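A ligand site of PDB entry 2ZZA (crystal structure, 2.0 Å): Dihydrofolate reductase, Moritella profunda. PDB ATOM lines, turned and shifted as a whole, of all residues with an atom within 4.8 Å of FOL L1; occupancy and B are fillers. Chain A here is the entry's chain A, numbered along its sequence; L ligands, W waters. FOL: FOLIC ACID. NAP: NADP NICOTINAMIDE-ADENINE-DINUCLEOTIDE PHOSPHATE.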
ATOM      1  N   ILE A   6      -7.277 -20.473  -3.857  1.00  0.00           N
ATOM      2  CA  ILE A   6      -8.223 -19.380  -3.705  1.00  0.00           C
ATOM      3  C   ILE A   6      -9.247 -19.711  -2.629  1.00  0.00           C
ATOM      4  O   ILE A   6      -9.805 -20.804  -2.604  1.00  0.00           O
ATOM      5  CB  ILE A   6      -8.914 -19.048  -5.055  1.00  0.00           C
ATOM      6  CG1 ILE A   6      -9.977 -17.963  -4.854  1.00  0.00           C
ATOM      7  CG2 ILE A   6      -9.491 -20.315  -5.675  1.00  0.00           C
ATOM      8  CD1 ILE A   6     -10.415 -17.281  -6.161  1.00  0.00           C
ATOM      9  N   ALA A   7      -9.479 -18.752  -1.728  1.00  0.00           N
ATOM     10  CA  ALA A   7     -10.426 -18.938  -0.648  1.00  0.00           C
ATOM     11  C   ALA A   7     -10.923 -17.611  -0.101  1.00  0.00           C
ATOM     12  O   ALA A   7     -10.304 -16.583  -0.303  1.00  0.00           O
ATOM     13  CB  ALA A   7      -9.782 -19.735   0.478  1.00  0.00           C
ATOM     14  N   ALA A   8     -12.067 -17.659   0.593  1.00  0.00           N
ATOM     15  CA  ALA A   8     -12.647 -16.489   1.234  1.00  0.00           C
ATOM     16  C   ALA A   8     -12.745 -16.815   2.719  1.00  0.00           C
ATOM     17  O   ALA A   8     -13.476 -17.738   3.114  1.00  0.00           O
ATOM     18  CB  ALA A   8     -14.035 -16.200   0.661  1.00  0.00           C
ATOM     19  N   MET A  21     -20.980 -22.447   3.195  1.00  0.00           N
ATOM     20  CA  MET A  21     -20.276 -21.199   3.498  1.00  0.00           C
ATOM     21  C   MET A  21     -21.136 -20.514   4.560  1.00  0.00           C
ATOM     22  O   MET A  21     -22.356 -20.483   4.441  1.00  0.00           O
ATOM     23  CB  MET A  21     -20.218 -20.328   2.245  1.00  0.00           C
ATOM     24  CG  MET A  21     -19.643 -21.024   1.039  1.00  0.00           C
ATOM     25  SD  MET A  21     -17.902 -20.733   0.927  1.00  0.00           S
ATOM     26  CE  MET A  21     -17.900 -18.986   0.784  1.00  0.00           C
ATOM     27  N   GLU A  28     -18.955 -11.570  -4.215  1.00  0.00           N
ATOM     28  CA  GLU A  28     -17.684 -12.213  -3.896  1.00  0.00           C
ATOM     29  C   GLU A  28     -17.574 -13.534  -4.665  1.00  0.00           C
ATOM     30  O   GLU A  28     -16.490 -13.938  -5.073  1.00  0.00           O
ATOM     31  CB  GLU A  28     -17.565 -12.451  -2.380  1.00  0.00           C
ATOM     32  CG  GLU A  28     -16.132 -12.576  -1.895  1.00  0.00           C
ATOM     33  CD  GLU A  28     -15.480 -13.902  -2.260  1.00  0.00           C
ATOM     34  OE1 GLU A  28     -14.252 -13.910  -2.532  1.00  0.00           O
ATOM     35  OE2 GLU A  28     -16.194 -14.922  -2.262  1.00  0.00           O
ATOM     36  N   LEU A  29     -18.704 -14.213  -4.850  1.00  0.00           N
ATOM     37  CA  LEU A  29     -18.725 -15.470  -5.605  1.00  0.00           C
ATOM     38  C   LEU A  29     -18.381 -15.164  -7.071  1.00  0.00           C
ATOM     39  O   LEU A  29     -17.800 -15.987  -7.764  1.00  0.00           O
ATOM     40  CB  LEU A  29     -20.093 -16.126  -5.524  1.00  0.00           C
ATOM     41  CG  LEU A  29     -20.361 -16.963  -4.271  1.00  0.00           C
ATOM     42  CD1 LEU A  29     -21.768 -17.542  -4.316  1.00  0.00           C
ATOM     43  CD2 LEU A  29     -19.325 -18.070  -4.188  1.00  0.00           C
ATOM     44  N   GLN A  30     -18.757 -13.971  -7.533  1.00  0.00           N
ATOM     45  CA  GLN A  30     -18.451 -13.571  -8.901  1.00  0.00           C
ATOM     46  C   GLN A  30     -16.947 -13.290  -9.004  1.00  0.00           C
ATOM     47  O   GLN A  30     -16.352 -13.432 -10.059  1.00  0.00           O
ATOM     48  CB  GLN A  30     -19.259 -12.325  -9.290  1.00  0.00           C
ATOM     49  CG  GLN A  30     -20.732 -12.590  -9.558  1.00  0.00           C
ATOM     50  CD  GLN A  30     -20.949 -13.654 -10.629  1.00  0.00           C
ATOM     51  OE1 GLN A  30     -20.393 -13.566 -11.725  1.00  0.00           O
ATOM     52  NE2 GLN A  30     -21.781 -14.651 -10.323  1.00  0.00           N
ATOM     53  N   LEU A  31     -16.352 -12.881  -7.888  1.00  0.00           N
ATOM     54  CA  LEU A  31     -14.912 -12.626  -7.862  1.00  0.00           C
ATOM     55  C   LEU A  31     -14.222 -13.990  -7.969  1.00  0.00           C
ATOM     56  O   LEU A  31     -13.191 -14.142  -8.641  1.00  0.00           O
ATOM     57  CB  LEU A  31     -14.530 -11.909  -6.560  1.00  0.00           C
ATOM     58  CG  LEU A  31     -13.066 -11.554  -6.317  1.00  0.00           C
ATOM     59  CD1 LEU A  31     -12.980 -10.503  -5.222  1.00  0.00           C
ATOM     60  CD2 LEU A  31     -12.278 -12.791  -5.932  1.00  0.00           C
ATOM     61  N   PHE A  32     -14.790 -14.997  -7.318  1.00  0.00           N
ATOM     62  CA  PHE A  32     -14.263 -16.349  -7.371  1.00  0.00           C
ATOM     63  C   PHE A  32     -14.333 -16.848  -8.815  1.00  0.00           C
ATOM     64  O   PHE A  32     -13.369 -17.411  -9.341  1.00  0.00           O
ATOM     65  CB  PHE A  32     -15.086 -17.281  -6.490  1.00  0.00           C
ATOM     66  CG  PHE A  32     -14.752 -18.732  -6.665  1.00  0.00           C
ATOM     67  CD1 PHE A  32     -13.657 -19.301  -6.015  1.00  0.00           C
ATOM     68  CD2 PHE A  32     -15.533 -19.546  -7.494  1.00  0.00           C
ATOM     69  CE1 PHE A  32     -13.345 -20.662  -6.168  1.00  0.00           C
ATOM     70  CE2 PHE A  32     -15.221 -20.902  -7.655  1.00  0.00           C
ATOM     71  CZ  PHE A  32     -14.131 -21.458  -6.985  1.00  0.00           C
ATOM     72  N   LYS A  33     -15.482 -16.664  -9.446  1.00  0.00           N
ATOM     73  CA  LYS A  33     -15.665 -17.116 -10.817  1.00  0.00           C
ATOM     74  C   LYS A  33     -14.670 -16.405 -11.731  1.00  0.00           C
ATOM     75  O   LYS A  33     -14.085 -17.016 -12.610  1.00  0.00           O
ATOM     76  CB  LYS A  33     -17.093 -16.845 -11.304  1.00  0.00           C
ATOM     77  CG  LYS A  33     -17.338 -17.313 -12.717  1.00  0.00           C
ATOM     78  CD  LYS A  33     -18.721 -16.955 -13.210  1.00  0.00           C
ATOM     79  CE  LYS A  33     -18.902 -17.457 -14.638  1.00  0.00           C
ATOM     80  NZ  LYS A  33     -20.185 -17.007 -15.245  1.00  0.00           N
ATOM     81  N   THR A  47     -15.971 -30.412  -0.746  1.00  0.00           N
ATOM     82  CA  THR A  47     -16.210 -29.129  -1.396  1.00  0.00           C
ATOM     83  C   THR A  47     -17.042 -29.330  -2.661  1.00  0.00           C
ATOM     84  O   THR A  47     -17.946 -28.548  -2.961  1.00  0.00           O
ATOM     85  CB  THR A  47     -14.891 -28.421  -1.751  1.00  0.00           C
ATOM     86  OG1 THR A  47     -14.214 -28.045  -0.542  1.00  0.00           O
ATOM     87  CG2 THR A  47     -15.156 -27.163  -2.582  1.00  0.00           C
ATOM     88  N   SER A  50     -20.553 -29.741  -1.649  1.00  0.00           N
ATOM     89  CA  SER A  50     -21.140 -28.525  -1.097  1.00  0.00           C
ATOM     90  C   SER A  50     -21.548 -27.602  -2.240  1.00  0.00           C
ATOM     91  O   SER A  50     -22.542 -26.886  -2.160  1.00  0.00           O
ATOM     92  CB  SER A  50     -20.144 -27.800  -0.184  1.00  0.00           C
ATOM     93  OG  SER A  50     -19.099 -27.209  -0.928  1.00  0.00           O
ATOM     94  N   ILE A  51     -20.772 -27.621  -3.322  1.00  0.00           N
ATOM     95  CA  ILE A  51     -21.075 -26.789  -4.483  1.00  0.00           C
ATOM     96  C   ILE A  51     -22.345 -27.323  -5.150  1.00  0.00           C
ATOM     97  O   ILE A  51     -23.208 -26.545  -5.562  1.00  0.00           O
ATOM     98  CB  ILE A  51     -19.890 -26.797  -5.477  1.00  0.00           C
ATOM     99  CG1 ILE A  51     -18.703 -26.067  -4.834  1.00  0.00           C
ATOM    100  CG2 ILE A  51     -20.286 -26.113  -6.786  1.00  0.00           C
ATOM    101  CD1 ILE A  51     -17.460 -25.993  -5.696  1.00  0.00           C
ATOM    102  N   ARG A  53     -22.591 -29.240  -8.012  1.00  0.00           N
ATOM    103  CA  ARG A  53     -22.518 -29.521  -9.444  1.00  0.00           C
ATOM    104  C   ARG A  53     -21.199 -28.976  -9.986  1.00  0.00           C
ATOM    105  O   ARG A  53     -20.534 -28.181  -9.329  1.00  0.00           O
ATOM    106  CB  ARG A  53     -23.688 -28.871 -10.192  1.00  0.00           C
ATOM    107  CG  ARG A  53     -23.380 -27.527 -10.838  1.00  0.00           C
ATOM    108  CD  ARG A  53     -23.177 -26.442  -9.812  1.00  0.00           C
ATOM    109  NE  ARG A  53     -22.886 -25.151 -10.443  1.00  0.00           N
ATOM    110  CZ  ARG A  53     -23.421 -24.010 -10.048  1.00  0.00           C
ATOM    111  NH1 ARG A  53     -23.112 -22.870 -10.658  1.00  0.00           N
ATOM    112  NH2 ARG A  53     -24.285 -24.004  -9.041  1.00  0.00           N
ATOM    113  N   LEU A  55     -18.640 -26.666 -11.925  1.00  0.00           N
ATOM    114  CA  LEU A  55     -18.727 -25.257 -12.243  1.00  0.00           C
ATOM    115  C   LEU A  55     -18.433 -25.104 -13.732  1.00  0.00           C
ATOM    116  O   LEU A  55     -17.468 -25.659 -14.253  1.00  0.00           O
ATOM    117  CB  LEU A  55     -17.738 -24.452 -11.397  1.00  0.00           C
ATOM    118  CG  LEU A  55     -18.016 -24.477  -9.886  1.00  0.00           C
ATOM    119  CD1 LEU A  55     -16.913 -23.740  -9.139  1.00  0.00           C
ATOM    120  CD2 LEU A  55     -19.368 -23.833  -9.605  1.00  0.00           C
ATOM    121  N   PRO A  56     -19.280 -24.349 -14.444  1.00  0.00           N
ATOM    122  CA  PRO A  56     -19.121 -24.130 -15.883  1.00  0.00           C
ATOM    123  C   PRO A  56     -17.870 -23.386 -16.305  1.00  0.00           C
ATOM    124  O   PRO A  56     -17.357 -22.525 -15.585  1.00  0.00           O
ATOM    125  CB  PRO A  56     -20.401 -23.372 -16.246  1.00  0.00           C
ATOM    126  CG  PRO A  56     -20.663 -22.564 -15.012  1.00  0.00           C
ATOM    127  CD  PRO A  56     -20.426 -23.587 -13.922  1.00  0.00           C
ATOM    128  N   ARG A  58     -14.868 -24.433 -16.590  1.00  0.00           N
ATOM    129  CA  ARG A  58     -13.663 -24.835 -15.888  1.00  0.00           C
ATOM    130  C   ARG A  58     -13.545 -26.357 -15.870  1.00  0.00           C
ATOM    131  O   ARG A  58     -14.555 -27.060 -15.877  1.00  0.00           O
ATOM    132  CB  ARG A  58     -13.683 -24.323 -14.442  1.00  0.00           C
ATOM    133  CG  ARG A  58     -13.254 -22.866 -14.274  1.00  0.00           C
ATOM    134  CD  ARG A  58     -13.986 -22.190 -13.119  1.00  0.00           C
ATOM    135  NE  ARG A  58     -15.412 -22.036 -13.419  1.00  0.00           N
ATOM    136  CZ  ARG A  58     -16.289 -21.396 -12.647  1.00  0.00           C
ATOM    137  NH1 ARG A  58     -17.554 -21.317 -13.017  1.00  0.00           N
ATOM    138  NH2 ARG A  58     -15.898 -20.817 -11.517  1.00  0.00           N
ATOM    139  N   ILE A  96      -9.196 -24.870  -5.087  1.00  0.00           N
ATOM    140  CA  ILE A  96     -10.353 -24.249  -4.547  1.00  0.00           C
ATOM    141  C   ILE A  96     -10.904 -24.773  -3.219  1.00  0.00           C
ATOM    142  O   ILE A  96     -11.912 -24.461  -2.814  1.00  0.00           O
ATOM    143  CB  ILE A  96     -11.426 -24.149  -5.486  1.00  0.00           C
ATOM    144  CG1 ILE A  96     -12.035 -25.482  -5.694  1.00  0.00           C
ATOM    145  CG2 ILE A  96     -11.114 -23.397  -6.700  1.00  0.00           C
ATOM    146  CD1 ILE A  96     -13.101 -25.518  -6.162  1.00  0.00           C
ATOM    147  N   TYR A 102      -6.380 -27.384   1.142  1.00  0.00           N
ATOM    148  CA  TYR A 102      -5.569 -26.195   1.412  1.00  0.00           C
ATOM    149  C   TYR A 102      -4.411 -26.600   2.317  1.00  0.00           C
ATOM    150  O   TYR A 102      -3.266 -26.196   2.100  1.00  0.00           O
ATOM    151  CB  TYR A 102      -6.388 -25.114   2.130  1.00  0.00           C
ATOM    152  CG  TYR A 102      -7.521 -24.508   1.340  1.00  0.00           C
ATOM    153  CD1 TYR A 102      -7.348 -24.086   0.018  1.00  0.00           C
ATOM    154  CD2 TYR A 102      -8.766 -24.277   1.945  1.00  0.00           C
ATOM    155  CE1 TYR A 102      -8.367 -23.450  -0.677  1.00  0.00           C
ATOM    156  CE2 TYR A 102      -9.792 -23.637   1.265  1.00  0.00           C
ATOM    157  CZ  TYR A 102      -9.588 -23.231  -0.045  1.00  0.00           C
ATOM    158  OH  TYR A 102     -10.617 -22.624  -0.710  1.00  0.00           O
ATOM    159  N   THR A 115      -9.733 -13.616  -0.057  1.00  0.00           N
ATOM    160  CA  THR A 115     -10.741 -12.599   0.168  1.00  0.00           C
ATOM    161  C   THR A 115     -10.987 -12.621   1.679  1.00  0.00           C
ATOM    162  O   THR A 115     -11.410 -13.642   2.229  1.00  0.00           O
ATOM    163  CB  THR A 115     -12.062 -12.915  -0.534  1.00  0.00           C
ATOM    164  OG1 THR A 115     -11.890 -12.817  -1.956  1.00  0.00           O
ATOM    165  CG2 THR A 115     -13.129 -11.924  -0.084  1.00  0.00           C
HETATM  166  N1  FOL L   1     -13.156 -18.666  -2.824  1.00  0.00           N
HETATM  167  C2  FOL L   1     -13.684 -17.438  -2.707  1.00  0.00           C
HETATM  168  NA2 FOL L   1     -12.927 -16.361  -2.933  1.00  0.00           N
HETATM  169  N3  FOL L   1     -15.044 -17.290  -2.386  1.00  0.00           N
HETATM  170  C4  FOL L   1     -15.829 -18.431  -2.199  1.00  0.00           C
HETATM  171  O4  FOL L   1     -17.022 -18.327  -1.940  1.00  0.00           O
HETATM  172  C4A FOL L   1     -15.236 -19.679  -2.332  1.00  0.00           C
HETATM  173  N5  FOL L   1     -15.982 -20.791  -2.248  1.00  0.00           N
HETATM  174  C6  FOL L   1     -15.426 -21.988  -2.466  1.00  0.00           C
HETATM  175  C7  FOL L   1     -14.073 -22.062  -2.787  1.00  0.00           C
HETATM  176  N8  FOL L   1     -13.341 -20.970  -2.871  1.00  0.00           N
HETATM  177  C8A FOL L   1     -13.885 -19.766  -2.650  1.00  0.00           C
HETATM  178  C9  FOL L   1     -16.248 -23.267  -2.412  1.00  0.00           C
HETATM  179  N10 FOL L   1     -17.704 -23.005  -2.463  1.00  0.00           N
HETATM  180  C11 FOL L   1     -19.658 -21.641  -5.832  1.00  0.00           C
HETATM  181  C12 FOL L   1     -20.367 -21.917  -4.657  1.00  0.00           C
HETATM  182  C13 FOL L   1     -19.697 -22.381  -3.533  1.00  0.00           C
HETATM  183  C14 FOL L   1     -18.314 -22.572  -3.563  1.00  0.00           C
HETATM  184  C15 FOL L   1     -17.612 -22.292  -4.723  1.00  0.00           C
HETATM  185  C16 FOL L   1     -18.283 -21.822  -5.855  1.00  0.00           C
HETATM  186  C   FOL L   1     -20.395 -21.145  -7.073  1.00  0.00           C
HETATM  187  O   FOL L   1     -21.599 -21.391  -7.239  1.00  0.00           O
HETATM  188  N   FOL L   1     -19.654 -20.462  -7.943  1.00  0.00           N
HETATM  189  CA  FOL L   1     -20.203 -19.937  -9.201  1.00  0.00           C
HETATM  190  CB  FOL L   1     -20.589 -18.470  -9.047  1.00  0.00           C
HETATM  191  CG  FOL L   1     -21.834 -18.282  -8.160  1.00  0.00           C
HETATM  192  CD  FOL L   1     -23.089 -18.841  -8.832  1.00  0.00           C
HETATM  193  OE1 FOL L   1     -22.986 -19.174 -10.038  1.00  0.00           O
HETATM  194  OE2 FOL L   1     -24.123 -18.904  -8.143  1.00  0.00           O
HETATM  195  CT  FOL L   1     -19.110 -20.039 -10.273  1.00  0.00           C
HETATM  196  O1  FOL L   1     -17.932 -20.063  -9.875  1.00  0.00           O
HETATM  197  O2  FOL L   1     -19.492 -20.099 -11.464  1.00  0.00           O
HETATM  198  PA  NAP L   2     -12.583 -31.092   1.592  1.00  0.00           P
HETATM  199  O1A NAP L   2     -11.174 -30.670   1.811  1.00  0.00           O
HETATM  200  O2A NAP L   2     -13.313 -30.231   0.441  1.00  0.00           O
HETATM  201  O5B NAP L   2     -12.677 -32.613   1.101  1.00  0.00           O
HETATM  202  C5B NAP L   2     -12.120 -33.651   1.913  1.00  0.00           C
HETATM  203  C4B NAP L   2     -12.134 -34.982   1.158  1.00  0.00           C
HETATM  204  O4B NAP L   2     -11.365 -34.920  -0.051  1.00  0.00           O
HETATM  205  C3B NAP L   2     -11.477 -36.098   1.972  1.00  0.00           C
HETATM  206  O3B NAP L   2     -12.415 -36.586   2.931  1.00  0.00           O
HETATM  207  C2B NAP L   2     -11.315 -37.111   0.839  1.00  0.00           C
HETATM  208  O2B NAP L   2     -12.601 -37.592   0.445  1.00  0.00           O
HETATM  209  C1B NAP L   2     -10.762 -36.204  -0.267  1.00  0.00           C
HETATM  210  N9A NAP L   2      -9.302 -36.058  -0.134  1.00  0.00           N
HETATM  211  C8A NAP L   2      -8.657 -35.219   0.659  1.00  0.00           C
HETATM  212  N7A NAP L   2      -7.342 -35.338   0.466  1.00  0.00           N
HETATM  213  C5A NAP L   2      -7.151 -36.269  -0.462  1.00  0.00           C
HETATM  214  C6A NAP L   2      -6.034 -36.802  -1.086  1.00  0.00           C
HETATM  215  N6A NAP L   2      -4.813 -36.375  -0.770  1.00  0.00           N
HETATM  216  N1A NAP L   2      -6.198 -37.741  -2.033  1.00  0.00           N
HETATM  217  C2A NAP L   2      -7.401 -38.161  -2.369  1.00  0.00           C
HETATM  218  N3A NAP L   2      -8.494 -37.673  -1.799  1.00  0.00           N
HETATM  219  C4A NAP L   2      -8.400 -36.730  -0.845  1.00  0.00           C
HETATM  220  O3  NAP L   2     -13.526 -31.006   2.895  1.00  0.00           O
HETATM  221  PN  NAP L   2     -13.368 -29.921   4.078  1.00  0.00           P
HETATM  222  O1N NAP L   2     -14.396 -30.495   4.963  1.00  0.00           O
HETATM  223  O2N NAP L   2     -11.908 -30.033   4.296  1.00  0.00           O
HETATM  224  O5D NAP L   2     -13.799 -28.711   3.107  1.00  0.00           O
HETATM  225  C5D NAP L   2     -15.183 -28.408   2.899  1.00  0.00           C
HETATM  226  C4D NAP L   2     -15.663 -27.294   3.819  1.00  0.00           C
HETATM  227  O4D NAP L   2     -14.899 -26.122   3.476  1.00  0.00           O
HETATM  228  C3D NAP L   2     -17.127 -26.945   3.515  1.00  0.00           C
HETATM  229  O3D NAP L   2     -17.733 -26.251   4.603  1.00  0.00           O
HETATM  230  C2D NAP L   2     -16.960 -25.991   2.332  1.00  0.00           C
HETATM  231  O2D NAP L   2     -18.098 -25.135   2.214  1.00  0.00           O
HETATM  232  C1D NAP L   2     -15.785 -25.167   2.869  1.00  0.00           C
HETATM  233  N1N NAP L   2     -15.100 -24.376   1.811  1.00  0.00           N
HETATM  234  C2N NAP L   2     -14.969 -22.991   1.940  1.00  0.00           C
HETATM  235  C3N NAP L   2     -14.247 -22.281   0.994  1.00  0.00           C
HETATM  236  C7N NAP L   2     -14.080 -20.758   1.137  1.00  0.00           C
HETATM  237  O7N NAP L   2     -13.256 -20.149   0.465  1.00  0.00           O
HETATM  238  N7N NAP L   2     -14.873 -20.186   2.039  1.00  0.00           N
HETATM  239  C4N NAP L   2     -13.651 -22.939  -0.069  1.00  0.00           C
HETATM  240  C5N NAP L   2     -13.772 -24.320  -0.208  1.00  0.00           C
HETATM  241  C6N NAP L   2     -14.499 -25.047   0.727  1.00  0.00           C
HETATM  242  P2B NAP L   2     -12.823 -39.165   0.214  1.00  0.00           P
HETATM  243  O1X NAP L   2     -13.852 -39.441  -0.802  1.00  0.00           O
HETATM  244  O2X NAP L   2     -11.390 -39.784  -0.164  1.00  0.00           O
HETATM  245  O3X NAP L   2     -13.217 -39.744   1.674  1.00  0.00           O
HETATM  246  O   HOH W   1     -10.527 -14.906  -3.269  1.00  0.00           O
HETATM  247  O   HOH W   2     -18.143 -16.117  -0.778  1.00  0.00           O
HETATM  248  O   HOH W   3     -19.154 -24.467  -0.444  1.00  0.00           O
HETATM  249  O   HOH W   4     -21.812 -19.760 -12.590  1.00  0.00           O
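SD of Met 21 sits close to N5 of FOL L1.
NH2 of Arg 58 is in salt-bridge range of O1 of FOL L1, at 2.7 Å.
N of Thr 47 sits at hydrogen-bond distance from O2A of NAP L2, 2.9 Å away.
An oxygen (OE1) of FOL L1 is in salt-bridge range of the guanidinium group of Arg 53 (3.7 Å).
O of Ala 8 is in hydrogen-bond range of N7N of NAP L2.
The backbone NH (N) of Ala 8 lies within hydrogen-bond range of an oxygen (O7N) of NAP L2 (2.8 Å).
An oxygen (O2A) of NAP L2 lies within hydrogen-bond range of the side-chain hydroxyl of Thr 47 (2.6 Å).
OE2 of Glu 28 sits at hydrogen-bond distance from N3 of FOL L1, 2.6 Å away.
N7N of NAP L2 is in hydrogen-bond range of SD of Met 21, 3.3 Å away.
A nitrogen (N8) of FOL L1 lies close to an oxygen (O7N) of NAP L2, at 3.4 Å.
O of Ala 7 is in hydrogen-bond range of N of Thr 115 (3.0 Å).
The backbone carbonyl oxygen (O) of Ile 6 lies within hydrogen-bond range of the side-chain hydroxyl (OH) of Tyr 102, at 2.7 Å.
The guanidinium group of Arg 58 lies within hydrogen-bond range of the backbone carbonyl oxygen of Pro 56.
The side-chain hydroxyl of Thr 115 sits at hydrogen-bond distance from the side-chain carboxylate of Glu 28, at 2.7 Å.
OH of Tyr 102 is in hydrogen-bond range of O of Ile 96 (3.1 Å).
Ile 6 touches FOL L1 (O to N8, 3.5 Å).
CA of Ala 7 touches N1 of FOL L1, at 3.5 Å.
Ala 8 touches FOL L1.
CD2 of Leu 29 touches O4 of FOL L1, at 3.2 Å.
Phe 32 touches FOL L1 (CD1 to N1, 3.3 Å).
CB of Lys 33 touches O1 of FOL L1 (3.6 Å).
CG1 of Ile 51 touches C14 of FOL L1, at 3.7 Å.
Leu 55 touches FOL L1 (CD2 to N, 3.8 Å).
Ile 96 touches FOL L1 (O to C7, 3.2 Å).
Tyr 102 touches FOL L1.
OG1 of Thr 115 touches NA2 of FOL L1, 3.8 Å away.
Hydrophobic or aromatic side chains within 4 Å of FOL L1: Ile 6, Ala 8, Met 21, Leu 29, Phe 32, Ile 51 and Leu 55.
15 residues have an atom within 4 Å of FOL L1: Ile 6, Ala 7, Ala 8, Met 21, Glu 28, Leu 29, Phe 32, Lys 33, Ile 51, Arg 53, Leu 55, Arg 58, Ile 96, Tyr 102 and Thr 115.
The nearest printed residue that does not touch FOL L1 is Thr 47 (4.05 Å).
Water W2 lies within hydrogen-bond range of OE2 of Glu 28 (2.7 Å) and O4 of FOL L1 (2.7 Å).
Water W1 lies within hydrogen-bond range of the side-chain hydroxyl (OG1) of Thr 115 (2.8 Å), a nitrogen (NA2) of FOL L1 (2.8 Å) and the backbone carbonyl oxygen (O) of Ala 7 (3.4 Å).
Water W3 lies within hydrogen-bond range of OG of Ser 50 (2.8 Å), N10 of FOL L1 (2.9 Å) and O2D of NAP L2 (2.9 Å).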
